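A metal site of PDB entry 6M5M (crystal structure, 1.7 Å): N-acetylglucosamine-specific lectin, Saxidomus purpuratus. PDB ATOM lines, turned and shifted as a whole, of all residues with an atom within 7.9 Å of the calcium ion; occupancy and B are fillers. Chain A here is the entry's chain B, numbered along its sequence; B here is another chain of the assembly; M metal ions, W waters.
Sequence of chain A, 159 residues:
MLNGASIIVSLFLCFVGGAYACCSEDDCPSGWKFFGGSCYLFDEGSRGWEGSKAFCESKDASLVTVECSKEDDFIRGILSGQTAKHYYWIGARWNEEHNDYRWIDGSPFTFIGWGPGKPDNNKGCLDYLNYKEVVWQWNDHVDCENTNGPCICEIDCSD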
ATOM      1  N   PHE A  35       2.462   0.126 -22.790  1.00  0.00           N
ATOM      2  CA  PHE A  35       1.954   1.272 -23.567  1.00  0.00           C
ATOM      3  C   PHE A  35       0.716   1.887 -22.930  1.00  0.00           C
ATOM      4  O   PHE A  35      -0.196   1.152 -22.594  1.00  0.00           O
ATOM      5  CB  PHE A  35       1.542   0.899 -24.992  1.00  0.00           C
ATOM      6  CG  PHE A  35       1.064   2.105 -25.732  1.00  0.00           C
ATOM      7  CD1 PHE A  35       1.973   3.020 -26.255  1.00  0.00           C
ATOM      8  CD2 PHE A  35      -0.295   2.406 -25.820  1.00  0.00           C
ATOM      9  CE1 PHE A  35       1.546   4.157 -26.915  1.00  0.00           C
ATOM     10  CE2 PHE A  35      -0.722   3.552 -26.476  1.00  0.00           C
ATOM     11  CZ  PHE A  35       0.195   4.429 -27.013  1.00  0.00           C
ATOM     12  N   GLY A  36       0.639   3.216 -22.847  1.00  0.00           N
ATOM     13  CA  GLY A  36      -0.608   3.901 -22.470  1.00  0.00           C
ATOM     14  C   GLY A  36      -1.247   3.317 -21.218  1.00  0.00           C
ATOM     15  O   GLY A  36      -2.483   3.126 -21.187  1.00  0.00           O
ATOM     16  N   GLY A  37      -0.448   3.020 -20.205  1.00  0.00           N
ATOM     17  CA  GLY A  37      -0.961   2.532 -18.903  1.00  0.00           C
ATOM     18  C   GLY A  37      -1.518   1.118 -18.983  1.00  0.00           C
ATOM     19  O   GLY A  37      -2.286   0.688 -18.077  1.00  0.00           O
ATOM     20  N   SER A  38      -1.098   0.368 -19.989  1.00  0.00           N
ATOM     21  CA  SER A  38      -1.433  -1.058 -20.155  1.00  0.00           C
ATOM     22  C   SER A  38      -0.157  -1.855 -20.399  1.00  0.00           C
ATOM     23  O   SER A  38       0.816  -1.265 -20.981  1.00  0.00           O
ATOM     24  CB  SER A  38      -2.406  -1.209 -21.306  1.00  0.00           C
ATOM     25  OG  SER A  38      -3.695  -0.793 -20.887  1.00  0.00           O
ATOM     26  N   TYR A  40       0.917  -5.406 -22.426  1.00  0.00           N
ATOM     27  CA  TYR A  40       0.420  -6.240 -23.541  1.00  0.00           C
ATOM     28  C   TYR A  40       1.313  -7.464 -23.736  1.00  0.00           C
ATOM     29  O   TYR A  40       2.576  -7.345 -23.753  1.00  0.00           O
ATOM     30  CB  TYR A  40       0.366  -5.410 -24.817  1.00  0.00           C
ATOM     31  CG  TYR A  40      -0.506  -4.184 -24.728  1.00  0.00           C
ATOM     32  CD1 TYR A  40      -0.056  -3.004 -24.180  1.00  0.00           C
ATOM     33  CD2 TYR A  40      -1.802  -4.216 -25.210  1.00  0.00           C
ATOM     34  CE1 TYR A  40      -0.871  -1.888 -24.094  1.00  0.00           C
ATOM     35  CE2 TYR A  40      -2.623  -3.103 -25.140  1.00  0.00           C
ATOM     36  CZ  TYR A  40      -2.161  -1.930 -24.602  1.00  0.00           C
ATOM     37  OH  TYR A  40      -2.972  -0.850 -24.508  1.00  0.00           O
ATOM     38  N   LEU A  63      -8.215 -10.742 -23.366  1.00  0.00           N
ATOM     39  CA  LEU A  63      -8.031 -10.340 -24.776  1.00  0.00           C
ATOM     40  C   LEU A  63      -8.139  -8.821 -24.852  1.00  0.00           C
ATOM     41  O   LEU A  63      -8.930  -8.221 -24.132  1.00  0.00           O
ATOM     42  CB  LEU A  63      -9.073 -11.069 -25.626  1.00  0.00           C
ATOM     43  CG  LEU A  63      -8.733 -12.517 -25.952  1.00  0.00           C
ATOM     44  CD1 LEU A  63      -9.910 -13.211 -26.572  1.00  0.00           C
ATOM     45  CD2 LEU A  63      -7.525 -12.584 -26.892  1.00  0.00           C
ATOM     46  N   VAL A  64      -7.268  -8.204 -25.618  1.00  0.00           N
ATOM     47  CA  VAL A  64      -7.102  -6.733 -25.572  1.00  0.00           C
ATOM     48  C   VAL A  64      -8.396  -6.037 -25.972  1.00  0.00           C
ATOM     49  O   VAL A  64      -9.155  -6.550 -26.779  1.00  0.00           O
ATOM     50  CB  VAL A  64      -5.977  -6.298 -26.510  1.00  0.00           C
ATOM     51  CG1 VAL A  64      -6.316  -6.624 -27.946  1.00  0.00           C
ATOM     52  CG2 VAL A  64      -5.702  -4.831 -26.336  1.00  0.00           C
ATOM     53  N   THR A  65      -8.614  -4.871 -25.380  1.00  0.00           N
ATOM     54  CA  THR A  65      -9.754  -3.937 -25.682  1.00  0.00           C
ATOM     55  C   THR A  65      -9.104  -2.614 -26.077  1.00  0.00           C
ATOM     56  O   THR A  65      -8.125  -2.203 -25.395  1.00  0.00           O
ATOM     57  CB  THR A  65     -10.723  -3.841 -24.496  1.00  0.00           C
ATOM     58  OG1 THR A  65     -10.032  -3.331 -23.349  1.00  0.00           O
ATOM     59  CG2 THR A  65     -11.379  -5.164 -24.150  1.00  0.00           C
ATOM     60  N   VAL A  66      -9.557  -1.995 -27.173  1.00  0.00           N
ATOM     61  CA  VAL A  66      -8.883  -0.829 -27.809  1.00  0.00           C
ATOM     62  C   VAL A  66      -9.825   0.363 -27.713  1.00  0.00           C
ATOM     63  O   VAL A  66     -10.816   0.441 -28.464  1.00  0.00           O
ATOM     64  CB  VAL A  66      -8.488  -1.183 -29.249  1.00  0.00           C
ATOM     65  CG1 VAL A  66      -7.566  -0.151 -29.867  1.00  0.00           C
ATOM     66  CG2 VAL A  66      -7.852  -2.574 -29.298  1.00  0.00           C
ATOM     67  N   GLU A  67      -9.501   1.289 -26.826  1.00  0.00           N
ATOM     68  CA  GLU A  67     -10.459   2.354 -26.413  1.00  0.00           C
ATOM     69  C   GLU A  67     -10.197   3.640 -27.201  1.00  0.00           C
ATOM     70  O   GLU A  67     -11.092   4.504 -27.183  1.00  0.00           O
ATOM     71  CB  GLU A  67     -10.357   2.513 -24.903  1.00  0.00           C
ATOM     72  CG  GLU A  67     -11.092   1.393 -24.143  1.00  0.00           C
ATOM     73  CD  GLU A  67     -10.204   0.208 -23.752  1.00  0.00           C
ATOM     74  OE1 GLU A  67      -8.968   0.327 -23.894  1.00  0.00           O
ATOM     75  OE2 GLU A  67     -10.756  -0.811 -23.284  1.00  0.00           O
ATOM     76  N   CYS A  68      -9.034   3.771 -27.843  1.00  0.00           N
ATOM     77  CA  CYS A  68      -8.609   5.007 -28.526  1.00  0.00           C
ATOM     78  C   CYS A  68      -7.617   4.736 -29.663  1.00  0.00           C
ATOM     79  O   CYS A  68      -7.033   3.615 -29.752  1.00  0.00           O
ATOM     80  CB  CYS A  68      -7.944   5.955 -27.533  1.00  0.00           C
ATOM     81  SG  CYS A  68      -6.354   5.323 -26.921  1.00  0.00           S
ATOM     82  N   GLU A  71      -3.826   3.623 -28.948  1.00  0.00           N
ATOM     83  CA  GLU A  71      -3.700   2.183 -28.603  1.00  0.00           C
ATOM     84  C   GLU A  71      -3.769   1.356 -29.883  1.00  0.00           C
ATOM     85  O   GLU A  71      -3.019   0.394 -29.995  1.00  0.00           O
ATOM     86  CB  GLU A  71      -4.769   1.787 -27.584  1.00  0.00           C
ATOM     87  CG  GLU A  71      -4.555   0.401 -26.968  1.00  0.00           C
ATOM     88  CD  GLU A  71      -5.608   0.066 -25.939  1.00  0.00           C
ATOM     89  OE1 GLU A  71      -6.653   0.722 -25.983  1.00  0.00           O
ATOM     90  OE2 GLU A  71      -5.408  -0.869 -25.079  1.00  0.00           O
ATOM     91  N   ILE A  75      -0.685  -0.995 -31.295  1.00  0.00           N
ATOM     92  CA  ILE A  75      -0.881  -2.407 -31.749  1.00  0.00           C
ATOM     93  C   ILE A  75      -0.395  -2.585 -33.197  1.00  0.00           C
ATOM     94  O   ILE A  75       0.321  -3.548 -33.481  1.00  0.00           O
ATOM     95  CB  ILE A  75      -2.332  -2.879 -31.560  1.00  0.00           C
ATOM     96  CG1 ILE A  75      -2.711  -2.903 -30.081  1.00  0.00           C
ATOM     97  CG2 ILE A  75      -2.527  -4.252 -32.180  1.00  0.00           C
ATOM     98  CD1 ILE A  75      -4.175  -2.944 -29.804  1.00  0.00           C
ATOM     99  N   TRP A 103     -16.978  -4.990 -26.921  1.00  0.00           N
ATOM    100  CA  TRP A 103     -15.902  -5.657 -26.151  1.00  0.00           C
ATOM    101  C   TRP A 103     -16.495  -6.754 -25.251  1.00  0.00           C
ATOM    102  O   TRP A 103     -17.703  -6.706 -24.868  1.00  0.00           O
ATOM    103  CB  TRP A 103     -15.047  -4.616 -25.405  1.00  0.00           C
ATOM    104  CG  TRP A 103     -14.410  -3.579 -26.270  1.00  0.00           C
ATOM    105  CD1 TRP A 103     -14.642  -2.231 -26.222  1.00  0.00           C
ATOM    106  CD2 TRP A 103     -13.459  -3.764 -27.327  1.00  0.00           C
ATOM    107  NE1 TRP A 103     -13.934  -1.572 -27.200  1.00  0.00           N
ATOM    108  CE2 TRP A 103     -13.209  -2.505 -27.902  1.00  0.00           C
ATOM    109  CE3 TRP A 103     -12.864  -4.885 -27.893  1.00  0.00           C
ATOM    110  CZ2 TRP A 103     -12.324  -2.313 -28.971  1.00  0.00           C
ATOM    111  CZ3 TRP A 103     -11.973  -4.710 -28.921  1.00  0.00           C
ATOM    112  CH2 TRP A 103     -11.722  -3.446 -29.459  1.00  0.00           C
ATOM    113  N   GLU A 154      -4.120  -8.235 -22.588  1.00  0.00           N
ATOM    114  CA  GLU A 154      -3.897  -6.903 -21.976  1.00  0.00           C
ATOM    115  C   GLU A 154      -4.166  -6.975 -20.466  1.00  0.00           C
ATOM    116  O   GLU A 154      -5.222  -7.491 -20.099  1.00  0.00           O
ATOM    117  CB  GLU A 154      -4.799  -5.891 -22.697  1.00  0.00           C
ATOM    118  CG  GLU A 154      -4.605  -4.459 -22.189  1.00  0.00           C
ATOM    119  CD  GLU A 154      -5.685  -3.461 -22.590  1.00  0.00           C
ATOM    120  OE1 GLU A 154      -6.761  -3.910 -23.104  1.00  0.00           O
ATOM    121  OE2 GLU A 154      -5.476  -2.225 -22.309  1.00  0.00           O
ATOM    122  N   ILE A 155      -3.298  -6.366 -19.660  1.00  0.00           N
ATOM    123  CA  ILE A 155      -3.500  -6.061 -18.218  1.00  0.00           C
ATOM    124  C   ILE A 155      -3.504  -4.525 -18.136  1.00  0.00           C
ATOM    125  O   ILE A 155      -2.475  -3.925 -18.546  1.00  0.00           O
ATOM    126  CB  ILE A 155      -2.390  -6.702 -17.334  1.00  0.00           C
ATOM    127  CG1 ILE A 155      -2.227  -8.200 -17.584  1.00  0.00           C
ATOM    128  CG2 ILE A 155      -2.663  -6.434 -15.853  1.00  0.00           C
ATOM    129  CD1 ILE A 155      -0.941  -8.812 -17.002  1.00  0.00           C
ATOM    130  N   ASP A 156      -4.609  -3.903 -17.701  1.00  0.00           N
ATOM    131  CA  ASP A 156      -4.732  -2.415 -17.704  1.00  0.00           C
ATOM    132  C   ASP A 156      -4.826  -1.883 -16.264  1.00  0.00           C
ATOM    133  O   ASP A 156      -4.919  -0.643 -16.100  1.00  0.00           O
ATOM    134  CB  ASP A 156      -5.834  -1.973 -18.682  1.00  0.00           C
ATOM    135  CG  ASP A 156      -7.256  -2.292 -18.222  1.00  0.00           C
ATOM    136  OD1 ASP A 156      -7.410  -2.886 -17.124  1.00  0.00           O
ATOM    137  OD2 ASP A 156      -8.217  -1.914 -18.961  1.00  0.00           O
ATOM    138  N   LYS B  24      -7.824   5.521 -21.880  1.00  0.00           N
ATOM    139  CA  LYS B  24      -8.270   5.196 -20.507  1.00  0.00           C
ATOM    140  C   LYS B  24      -7.399   5.882 -19.450  1.00  0.00           C
ATOM    141  O   LYS B  24      -7.895   6.036 -18.347  1.00  0.00           O
ATOM    142  CB  LYS B  24      -8.184   3.692 -20.238  1.00  0.00           C
ATOM    143  CG  LYS B  24      -9.391   2.882 -20.667  1.00  0.00           C
ATOM    144  CD  LYS B  24      -9.480   1.510 -20.015  1.00  0.00           C
ATOM    145  CE  LYS B  24      -9.747   1.564 -18.520  1.00  0.00           C
ATOM    146  NZ  LYS B  24     -10.128   0.234 -17.999  1.00  0.00           N
HETATM  147 CA    CA M   1      -7.063  -1.126 -23.669  1.00  0.00          CA
HETATM  148  O   HOH W   1      -8.385  -1.582 -21.770  1.00  0.00           O
HETATM  149  O   HOH W   2      -6.339   0.721 -22.489  1.00  0.00           O
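OH of Tyr 40 sits close to OE2 of Glu 71, 2.5 Å away.
The side-chain sulfur (SG) of Cys 68 is in hydrogen-bond range of the backbone NH (N) of Glu 71, 3.7 Å away.
OE2 of Glu 154 lies close to OG of Ser 38 (2.7 Å).
The calcium ion is bound by the side-chain carboxylate (OE2) of Glu 71.
The backbone carbonyl oxygen (O) of Thr 65 binds the calcium ion, 2.3 Å away.
Water W2 is bound to the calcium ion (2.3 Å).
The calcium ion is bound by water W1.
The side-chain carboxylate (OE2) of Glu 154 binds the calcium ion (2.4 Å).
The calcium ion is bound by OE1 of Glu 67, 2.4 Å away.
The calcium ion is bound by OE1 of Glu 154, 2.9 Å away.
Slightly farther from the calcium ion lies the side-chain carboxylate (OE1) of Glu 71 (3.0 Å).
Water W1 lies within hydrogen-bond range of the side-chain carboxylate (OD2) of Asp 156, the side-chain hydroxyl (OG1) of Thr 65 and the side-chain carboxylate (OE2) of Glu 67.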
